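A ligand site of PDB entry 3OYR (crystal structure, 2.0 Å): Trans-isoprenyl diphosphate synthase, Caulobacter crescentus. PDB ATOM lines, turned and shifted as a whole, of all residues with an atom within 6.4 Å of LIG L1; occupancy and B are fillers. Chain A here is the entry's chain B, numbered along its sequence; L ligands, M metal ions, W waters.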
ATOM      1  N   GLY A  64     -21.964  15.274  -4.765  1.00  0.00           N
ATOM      2  CA  GLY A  64     -20.783  15.212  -3.922  1.00  0.00           C
ATOM      3  C   GLY A  64     -19.558  15.649  -4.688  1.00  0.00           C
ATOM      4  O   GLY A  64     -19.639  16.467  -5.628  1.00  0.00           O
ATOM      5  N   GLY A  65     -18.413  15.107  -4.302  1.00  0.00           N
ATOM      6  CA  GLY A  65     -17.162  15.375  -4.975  1.00  0.00           C
ATOM      7  C   GLY A  65     -16.265  16.124  -4.034  1.00  0.00           C
ATOM      8  O   GLY A  65     -16.721  16.982  -3.291  1.00  0.00           O
ATOM      9  N   LYS A  66     -14.978  15.808  -4.070  1.00  0.00           N
ATOM     10  CA  LYS A  66     -14.034  16.335  -3.071  1.00  0.00           C
ATOM     11  C   LYS A  66     -13.591  17.753  -3.354  1.00  0.00           C
ATOM     12  O   LYS A  66     -12.996  18.383  -2.482  1.00  0.00           O
ATOM     13  CB  LYS A  66     -12.823  15.411  -2.947  1.00  0.00           C
ATOM     14  CG  LYS A  66     -13.160  14.000  -2.490  1.00  0.00           C
ATOM     15  CD  LYS A  66     -11.905  13.096  -2.512  1.00  0.00           C
ATOM     16  CE  LYS A  66     -11.357  12.873  -3.949  1.00  0.00           C
ATOM     17  NZ  LYS A  66     -12.304  12.001  -4.737  1.00  0.00           N
ATOM     18  N   ARG A  67     -13.855  18.253  -4.570  1.00  0.00           N
ATOM     19  CA  ARG A  67     -13.509  19.624  -4.954  1.00  0.00           C
ATOM     20  C   ARG A  67     -12.016  19.924  -4.835  1.00  0.00           C
ATOM     21  O   ARG A  67     -11.640  21.073  -4.633  1.00  0.00           O
ATOM     22  CB  ARG A  67     -14.347  20.637  -4.166  1.00  0.00           C
ATOM     23  CG  ARG A  67     -15.850  20.410  -4.339  1.00  0.00           C
ATOM     24  CD  ARG A  67     -16.302  20.882  -5.733  1.00  0.00           C
ATOM     25  NE  ARG A  67     -17.759  20.951  -5.803  1.00  0.00           N
ATOM     26  CZ  ARG A  67     -18.534  19.905  -6.095  1.00  0.00           C
ATOM     27  NH1 ARG A  67     -18.002  18.720  -6.354  1.00  0.00           N
ATOM     28  NH2 ARG A  67     -19.849  20.057  -6.103  1.00  0.00           N
ATOM     29  N   LEU A  68     -11.183  18.890  -5.006  1.00  0.00           N
ATOM     30  CA  LEU A  68      -9.726  19.042  -4.855  1.00  0.00           C
ATOM     31  C   LEU A  68      -9.151  19.996  -5.881  1.00  0.00           C
ATOM     32  O   LEU A  68      -8.259  20.797  -5.568  1.00  0.00           O
ATOM     33  CB  LEU A  68      -9.000  17.686  -4.951  1.00  0.00           C
ATOM     34  CG  LEU A  68      -9.363  16.618  -3.905  1.00  0.00           C
ATOM     35  CD1 LEU A  68      -8.418  15.448  -3.988  1.00  0.00           C
ATOM     36  CD2 LEU A  68      -9.358  17.189  -2.483  1.00  0.00           C
ATOM     37  N   ARG A  69      -9.692  19.934  -7.096  1.00  0.00           N
ATOM     38  CA  ARG A  69      -9.204  20.802  -8.142  1.00  0.00           C
ATOM     39  C   ARG A  69      -9.415  22.303  -7.884  1.00  0.00           C
ATOM     40  O   ARG A  69      -8.401  23.039  -7.912  1.00  0.00           O
ATOM     41  CB  ARG A  69      -9.643  20.333  -9.515  1.00  0.00           C
ATOM     42  CG  ARG A  69      -8.961  19.052  -9.940  1.00  0.00           C
ATOM     43  CD  ARG A  69      -9.873  18.334 -10.872  1.00  0.00           C
ATOM     44  NE  ARG A  69      -9.459  16.964 -11.158  1.00  0.00           N
ATOM     45  CZ  ARG A  69      -9.841  15.912 -10.448  1.00  0.00           C
ATOM     46  NH1 ARG A  69     -10.626  16.059  -9.368  1.00  0.00           N
ATOM     47  NH2 ARG A  69      -9.408  14.717 -10.799  1.00  0.00           N
ATOM     48  N   GLU A  95     -13.500  23.319 -11.899  1.00  0.00           N
ATOM     49  CA  GLU A  95     -14.502  22.321 -11.498  1.00  0.00           C
ATOM     50  C   GLU A  95     -15.475  21.991 -12.613  1.00  0.00           C
ATOM     51  O   GLU A  95     -15.886  20.828 -12.741  1.00  0.00           O
ATOM     52  CB  GLU A  95     -15.266  22.717 -10.220  1.00  0.00           C
ATOM     53  CG  GLU A  95     -16.134  21.593  -9.575  1.00  0.00           C
ATOM     54  CD  GLU A  95     -15.346  20.342  -9.149  1.00  0.00           C
ATOM     55  OE1 GLU A  95     -14.108  20.387  -8.993  1.00  0.00           O
ATOM     56  OE2 GLU A  95     -15.969  19.294  -8.933  1.00  0.00           O
ATOM     57  N   HIS A  98     -13.606  19.742 -14.968  1.00  0.00           N
ATOM     58  CA  HIS A  98     -13.605  18.424 -14.339  1.00  0.00           C
ATOM     59  C   HIS A  98     -14.975  17.730 -14.471  1.00  0.00           C
ATOM     60  O   HIS A  98     -15.055  16.575 -14.910  1.00  0.00           O
ATOM     61  CB  HIS A  98     -13.150  18.556 -12.879  1.00  0.00           C
ATOM     62  CG  HIS A  98     -13.337  17.318 -12.062  1.00  0.00           C
ATOM     63  ND1 HIS A  98     -12.722  16.115 -12.367  1.00  0.00           N
ATOM     64  CD2 HIS A  98     -14.018  17.102 -10.904  1.00  0.00           C
ATOM     65  CE1 HIS A  98     -13.047  15.210 -11.465  1.00  0.00           C
ATOM     66  NE2 HIS A  98     -13.826  15.776 -10.560  1.00  0.00           N
ATOM     67  N   THR A 101     -15.658  16.515 -17.968  1.00  0.00           N
ATOM     68  CA  THR A 101     -14.856  15.342 -18.332  1.00  0.00           C
ATOM     69  C   THR A 101     -15.449  14.086 -17.703  1.00  0.00           C
ATOM     70  O   THR A 101     -15.382  13.023 -18.307  1.00  0.00           O
ATOM     71  CB  THR A 101     -13.381  15.426 -17.878  1.00  0.00           C
ATOM     72  OG1 THR A 101     -13.328  15.386 -16.446  1.00  0.00           O
ATOM     73  CG2 THR A 101     -12.694  16.684 -18.416  1.00  0.00           C
ATOM     74  N   LEU A 102     -16.001  14.220 -16.503  1.00  0.00           N
ATOM     75  CA  LEU A 102     -16.752  13.124 -15.868  1.00  0.00           C
ATOM     76  C   LEU A 102     -17.941  12.641 -16.689  1.00  0.00           C
ATOM     77  O   LEU A 102     -18.107  11.430 -16.892  1.00  0.00           O
ATOM     78  CB  LEU A 102     -17.229  13.499 -14.467  1.00  0.00           C
ATOM     79  CG  LEU A 102     -16.147  13.838 -13.447  1.00  0.00           C
ATOM     80  CD1 LEU A 102     -16.784  14.165 -12.119  1.00  0.00           C
ATOM     81  CD2 LEU A 102     -15.096  12.711 -13.296  1.00  0.00           C
ATOM     82  N   ARG A 114     -21.712   7.114 -10.254  1.00  0.00           N
ATOM     83  CA  ARG A 114     -20.809   8.246 -10.094  1.00  0.00           C
ATOM     84  C   ARG A 114     -21.267   9.061  -8.905  1.00  0.00           C
ATOM     85  O   ARG A 114     -22.424   9.510  -8.866  1.00  0.00           O
ATOM     86  CB  ARG A 114     -20.778   9.109 -11.369  1.00  0.00           C
ATOM     87  CG  ARG A 114     -20.047  10.460 -11.158  1.00  0.00           C
ATOM     88  CD  ARG A 114     -18.545  10.285 -11.014  1.00  0.00           C
ATOM     89  NE  ARG A 114     -17.958   9.774 -12.243  1.00  0.00           N
ATOM     90  CZ  ARG A 114     -16.699   9.377 -12.398  1.00  0.00           C
ATOM     91  NH1 ARG A 114     -15.838   9.437 -11.381  1.00  0.00           N
ATOM     92  NH2 ARG A 114     -16.307   8.937 -13.584  1.00  0.00           N
ATOM     93  N   ARG A 115     -20.352   9.226  -7.944  1.00  0.00           N
ATOM     94  CA  ARG A 115     -20.607   9.987  -6.712  1.00  0.00           C
ATOM     95  C   ARG A 115     -21.843   9.463  -5.944  1.00  0.00           C
ATOM     96  O   ARG A 115     -22.585  10.237  -5.327  1.00  0.00           O
ATOM     97  CB  ARG A 115     -20.722  11.492  -6.994  1.00  0.00           C
ATOM     98  CG  ARG A 115     -19.429  12.161  -7.478  1.00  0.00           C
ATOM     99  CD  ARG A 115     -19.667  13.643  -7.832  1.00  0.00           C
ATOM    100  NE  ARG A 115     -18.419  14.342  -8.189  1.00  0.00           N
ATOM    101  CZ  ARG A 115     -18.353  15.542  -8.761  1.00  0.00           C
ATOM    102  NH1 ARG A 115     -17.156  16.083  -9.034  1.00  0.00           N
ATOM    103  NH2 ARG A 115     -19.474  16.222  -9.068  1.00  0.00           N
ATOM    104  N   LYS A 191      -4.417  12.568 -18.945  1.00  0.00           N
ATOM    105  CA  LYS A 191      -5.840  12.518 -18.675  1.00  0.00           C
ATOM    106  C   LYS A 191      -6.185  12.977 -17.252  1.00  0.00           C
ATOM    107  O   LYS A 191      -7.312  13.392 -17.028  1.00  0.00           O
ATOM    108  CB  LYS A 191      -6.385  11.127 -18.941  1.00  0.00           C
ATOM    109  CG  LYS A 191      -6.265  10.180 -17.757  1.00  0.00           C
ATOM    110  CD  LYS A 191      -7.129   8.959 -17.942  1.00  0.00           C
ATOM    111  CE  LYS A 191      -6.828   7.956 -16.846  1.00  0.00           C
ATOM    112  NZ  LYS A 191      -7.722   6.754 -16.961  1.00  0.00           N
ATOM    113  N   THR A 192      -5.231  12.903 -16.320  1.00  0.00           N
ATOM    114  CA  THR A 192      -5.538  13.227 -14.922  1.00  0.00           C
ATOM    115  C   THR A 192      -4.602  14.247 -14.306  1.00  0.00           C
ATOM    116  O   THR A 192      -5.059  15.208 -13.695  1.00  0.00           O
ATOM    117  CB  THR A 192      -5.582  11.967 -14.046  1.00  0.00           C
ATOM    118  OG1 THR A 192      -6.604  11.085 -14.557  1.00  0.00           O
ATOM    119  CG2 THR A 192      -5.889  12.328 -12.588  1.00  0.00           C
ATOM    120  N   PHE A 196      -4.783  18.873 -12.604  1.00  0.00           N
ATOM    121  CA  PHE A 196      -4.212  19.229 -11.295  1.00  0.00           C
ATOM    122  C   PHE A 196      -3.083  20.230 -11.433  1.00  0.00           C
ATOM    123  O   PHE A 196      -3.067  21.215 -10.703  1.00  0.00           O
ATOM    124  CB  PHE A 196      -3.708  18.019 -10.521  1.00  0.00           C
ATOM    125  CG  PHE A 196      -4.802  17.249  -9.818  1.00  0.00           C
ATOM    126  CD1 PHE A 196      -5.223  16.016 -10.292  1.00  0.00           C
ATOM    127  CD2 PHE A 196      -5.400  17.753  -8.661  1.00  0.00           C
ATOM    128  CE1 PHE A 196      -6.219  15.311  -9.618  1.00  0.00           C
ATOM    129  CE2 PHE A 196      -6.387  17.067  -7.994  1.00  0.00           C
ATOM    130  CZ  PHE A 196      -6.793  15.836  -8.459  1.00  0.00           C
ATOM    131  N   PHE A 228      -2.313  10.803  -7.360  1.00  0.00           N
ATOM    132  CA  PHE A 228      -3.770  10.730  -7.267  1.00  0.00           C
ATOM    133  C   PHE A 228      -4.318   9.633  -8.158  1.00  0.00           C
ATOM    134  O   PHE A 228      -5.104   8.793  -7.698  1.00  0.00           O
ATOM    135  CB  PHE A 228      -4.403  12.092  -7.637  1.00  0.00           C
ATOM    136  CG  PHE A 228      -5.883  12.159  -7.383  1.00  0.00           C
ATOM    137  CD1 PHE A 228      -6.366  12.499  -6.114  1.00  0.00           C
ATOM    138  CD2 PHE A 228      -6.801  11.889  -8.409  1.00  0.00           C
ATOM    139  CE1 PHE A 228      -7.758  12.540  -5.868  1.00  0.00           C
ATOM    140  CE2 PHE A 228      -8.198  11.946  -8.170  1.00  0.00           C
ATOM    141  CZ  PHE A 228      -8.677  12.272  -6.904  1.00  0.00           C
ATOM    142  N   GLN A 229      -3.888   9.625  -9.417  1.00  0.00           N
ATOM    143  CA  GLN A 229      -4.415   8.667 -10.383  1.00  0.00           C
ATOM    144  C   GLN A 229      -3.945   7.231 -10.133  1.00  0.00           C
ATOM    145  O   GLN A 229      -4.736   6.275 -10.267  1.00  0.00           O
ATOM    146  CB  GLN A 229      -4.071   9.093 -11.800  1.00  0.00           C
ATOM    147  CG  GLN A 229      -4.766   8.258 -12.861  1.00  0.00           C
ATOM    148  CD  GLN A 229      -6.288   8.287 -12.735  1.00  0.00           C
ATOM    149  OE1 GLN A 229      -6.892   9.343 -12.579  1.00  0.00           O
ATOM    150  NE2 GLN A 229      -6.894   7.121 -12.798  1.00  0.00           N
ATOM    151  N   ASP A 232      -6.068   6.109  -7.439  1.00  0.00           N
ATOM    152  CA  ASP A 232      -7.380   5.846  -8.018  1.00  0.00           C
ATOM    153  C   ASP A 232      -7.422   4.502  -8.734  1.00  0.00           C
ATOM    154  O   ASP A 232      -8.387   3.745  -8.603  1.00  0.00           O
ATOM    155  CB  ASP A 232      -7.806   6.948  -8.992  1.00  0.00           C
ATOM    156  CG  ASP A 232      -9.213   6.751  -9.492  1.00  0.00           C
ATOM    157  OD1 ASP A 232      -9.393   6.164 -10.606  1.00  0.00           O
ATOM    158  OD2 ASP A 232     -10.156   7.134  -8.752  1.00  0.00           O
ATOM    159  N   LYS A 246     -18.473   4.920  -6.851  1.00  0.00           N
ATOM    160  CA  LYS A 246     -18.473   4.395  -8.212  1.00  0.00           C
ATOM    161  C   LYS A 246     -18.118   2.916  -8.091  1.00  0.00           C
ATOM    162  O   LYS A 246     -17.534   2.510  -7.092  1.00  0.00           O
ATOM    163  CB  LYS A 246     -17.470   5.162  -9.080  1.00  0.00           C
ATOM    164  CG  LYS A 246     -16.042   5.168  -8.555  1.00  0.00           C
ATOM    165  CD  LYS A 246     -15.170   6.246  -9.220  1.00  0.00           C
ATOM    166  CE  LYS A 246     -13.706   5.996  -8.975  1.00  0.00           C
ATOM    167  NZ  LYS A 246     -12.883   7.248  -9.150  1.00  0.00           N
ATOM    168  N   ARG A 343      -5.956   8.007   0.820  1.00  0.00           N
ATOM    169  CA  ARG A 343      -7.439   8.035   0.734  1.00  0.00           C
ATOM    170  C   ARG A 343      -8.111   6.715   0.325  1.00  0.00           C
ATOM    171  O   ARG A 343      -7.515   5.871  -0.351  1.00  0.00           O
ATOM    172  CB  ARG A 343      -7.900   9.134  -0.236  1.00  0.00           C
ATOM    173  CG  ARG A 343      -7.515   8.862  -1.663  1.00  0.00           C
ATOM    174  CD  ARG A 343      -7.396  10.116  -2.551  1.00  0.00           C
ATOM    175  NE  ARG A 343      -7.032   9.707  -3.913  1.00  0.00           N
ATOM    176  CZ  ARG A 343      -7.909   9.366  -4.857  1.00  0.00           C
ATOM    177  NH1 ARG A 343      -7.495   8.998  -6.062  1.00  0.00           N
ATOM    178  NH2 ARG A 343      -9.207   9.444  -4.595  1.00  0.00           N
ATOM    179  N   ALA A 345     -11.353   7.077  -0.972  1.00  0.00           N
ATOM    180  CA  ALA A 345     -12.314   7.561  -1.975  1.00  0.00           C
ATOM    181  C   ALA A 345     -11.829   8.841  -2.668  1.00  0.00           C
ATOM    182  O   ALA A 345     -10.884   9.497  -2.209  1.00  0.00           O
ATOM    183  CB  ALA A 345     -13.646   7.810  -1.338  1.00  0.00           C
ATOM    184  OXT ALA A 345     -12.411   9.239  -3.689  1.00  0.00           O
HETATM  185  C1  LIG L   1     -12.534  11.372 -10.653  1.00  0.00           C
HETATM  186  O1  LIG L   1     -12.047  12.472  -9.866  1.00  0.00           O
HETATM  187  C2  LIG L   1     -11.612  11.623 -11.804  1.00  0.00           C
HETATM  188  C3  LIG L   1     -10.431  10.996 -11.918  1.00  0.00           C
HETATM  189  C4  LIG L   1      -9.991   9.913 -10.972  1.00  0.00           C
HETATM  190  C5  LIG L   1      -9.565  11.417 -13.054  1.00  0.00           C
HETATM  191  P1  LIG L   1     -12.201  12.646  -8.285  1.00  0.00           P
HETATM  192  O2  LIG L   1     -11.518  13.915  -7.817  1.00  0.00           O
HETATM  193  O3  LIG L   1     -11.769  11.377  -7.619  1.00  0.00           O
HETATM  194  O4  LIG L   1     -13.816  12.791  -8.265  1.00  0.00           O
HETATM  195  P2  LIG L   1     -14.765  13.757  -7.360  1.00  0.00           P
HETATM  196  O5  LIG L   1     -14.743  15.113  -8.025  1.00  0.00           O
HETATM  197  O6  LIG L   1     -16.056  12.998  -7.590  1.00  0.00           O
HETATM  198  O7  LIG L   1     -14.260  13.761  -5.936  1.00  0.00           O
HETATM  199  C1  LG2 L   2     -10.099   9.290 -16.014  1.00  0.00           C
HETATM  200  O1  LG2 L   2      -9.888   8.387 -14.934  1.00  0.00           O
HETATM  201  C2  LG2 L   2     -11.371  10.072 -15.894  1.00  0.00           C
HETATM  202  C3  LG2 L   2     -11.442  11.379 -16.185  1.00  0.00           C
HETATM  203  C4  LG2 L   2     -10.279  12.189 -16.651  1.00  0.00           C
HETATM  204  C5  LG2 L   2     -12.775  12.027 -16.026  1.00  0.00           C
HETATM  205  P1  LG2 L   2     -10.839   7.109 -14.563  1.00  0.00           P
HETATM  206  O2  LG2 L   2      -9.923   6.200 -13.806  1.00  0.00           O
HETATM  207  O3  LG2 L   2     -11.621   6.597 -15.735  1.00  0.00           O
HETATM  208  O4  LG2 L   2     -11.820   7.861 -13.516  1.00  0.00           O
HETATM  209  P2  LG2 L   2     -13.115   7.228 -12.796  1.00  0.00           P
HETATM  210  O5  LG2 L   2     -13.425   8.383 -11.880  1.00  0.00           O
HETATM  211  O6  LG2 L   2     -12.638   5.958 -12.136  1.00  0.00           O
HETATM  212  O7  LG2 L   2     -14.135   6.943 -13.874  1.00  0.00           O
HETATM  213 CA    CA M   1     -10.708   4.913 -11.948  1.00  0.00          CA
HETATM  214  O   HOH W   1     -16.140  11.753  -4.760  1.00  0.00           O
HETATM  215  O   HOH W   2     -12.165  16.261  -6.574  1.00  0.00           O
HETATM  216  O   HOH W   3     -10.062   9.361  -7.314  1.00  0.00           O
HETATM  217  O   HOH W   4     -16.002  10.664  -8.586  1.00  0.00           O
HETATM  218  O   HOH W   5     -13.624   9.461  -7.677  1.00  0.00           O
HETATM  219  O   HOH W   6     -15.174  17.571  -7.033  1.00  0.00           O
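NH1 of Arg 69 lies close to NE2 of His 98, at 3.4 Å. The backbone carbonyl oxygen (O) of His 98 is in hydrogen-bond range of the side-chain hydroxyl (OG1) of Thr 101 (2.6 Å). NH1 of Arg 115 lies within salt-bridge range of OE2 of Glu 95, 3.4 Å away. NH2 of Arg 115 sits at hydrogen-bond distance from O of Gly 64 (3.5 Å). NH1 of Arg 343 sits at hydrogen-bond distance from O of Phe 228. The side-chain amide oxygen (OE1) of Gln 229 is in hydrogen-bond range of the side-chain hydroxyl (OG1) of Thr 192 (2.7 Å). The side-chain amide nitrogen (NE2) of Gln 229 sits close to the side-chain carboxylate (OD1) of Asp 232, at 3.5 Å. The side-chain amino group of Lys 246 lies within salt-bridge range of the side-chain carboxylate of Asp 232 (2.8 Å).
Water W4 bridges an oxygen (O6) of LIG L1 and the guanidinium group of Arg 114. Water W3 lies within hydrogen-bond range of OD2 of Asp 232 (2.7 Å), O3 of LIG L1 (2.7 Å) and NH2 of Arg 343 (2.9 Å). Water W5 bridges an oxygen (O3) of LIG L1 (2.7 Å) and the side-chain amino group of Lys 246 (2.8 Å).
Gly 65 touches LIG L1 (CA to O7, 3.5 Å). Leu 102 touches LIG L1. NH1 of Arg 114 touches C1 of LIG L1, 3.9 Å away. Thr 192 touches LIG L1 (OG1 to C5, 3.3 Å). Phe 228 touches LIG L1 (CZ to O3, 3.3 Å). Gln 229 touches LIG L1. Asp 232 touches LIG L1 (OD2 to C4, 3.6 Å). Hydrophobic or aromatic side chains that line LIG L1: His 98, Leu 102 and Phe 228. Of the 21 residues printed, 11 come within 4 Å of LIG L1. The nearest printed residue that does not touch LIG L1 is Lys 246 (4.3 Å).
A ring nitrogen (NE2) of His 98 lies within hydrogen-bond range of an oxygen (O5) of LIG L1 (2.8 Å). The guanidinium group of Arg 115 lies within salt-bridge range of an oxygen (O6) of LIG L1 (2.8 Å). An oxygen (O2) of LIG L1 lies within salt-bridge range of the guanidinium group (NH1) of Arg 69. N of Lys 66 is in hydrogen-bond range of O7 of LIG L1 (2.9 Å). O7 of LIG L1 is in salt-bridge range of NZ of Lys 66 (2.9 Å). NE2 of Gln 229 sits close to O2 of LG2 L2 (3.3 Å). The guanidinium group (NH1) of Arg 114 is in salt-bridge range of an oxygen (O5) of LG2 L2, 2.7 Å away. O5 of LG2 L2 lies within salt-bridge range of NZ of Lys 246. The side-chain amino group of Lys 191 is in hydrogen-bond range of an oxygen (O1) of LG2 L2 (3.4 Å).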
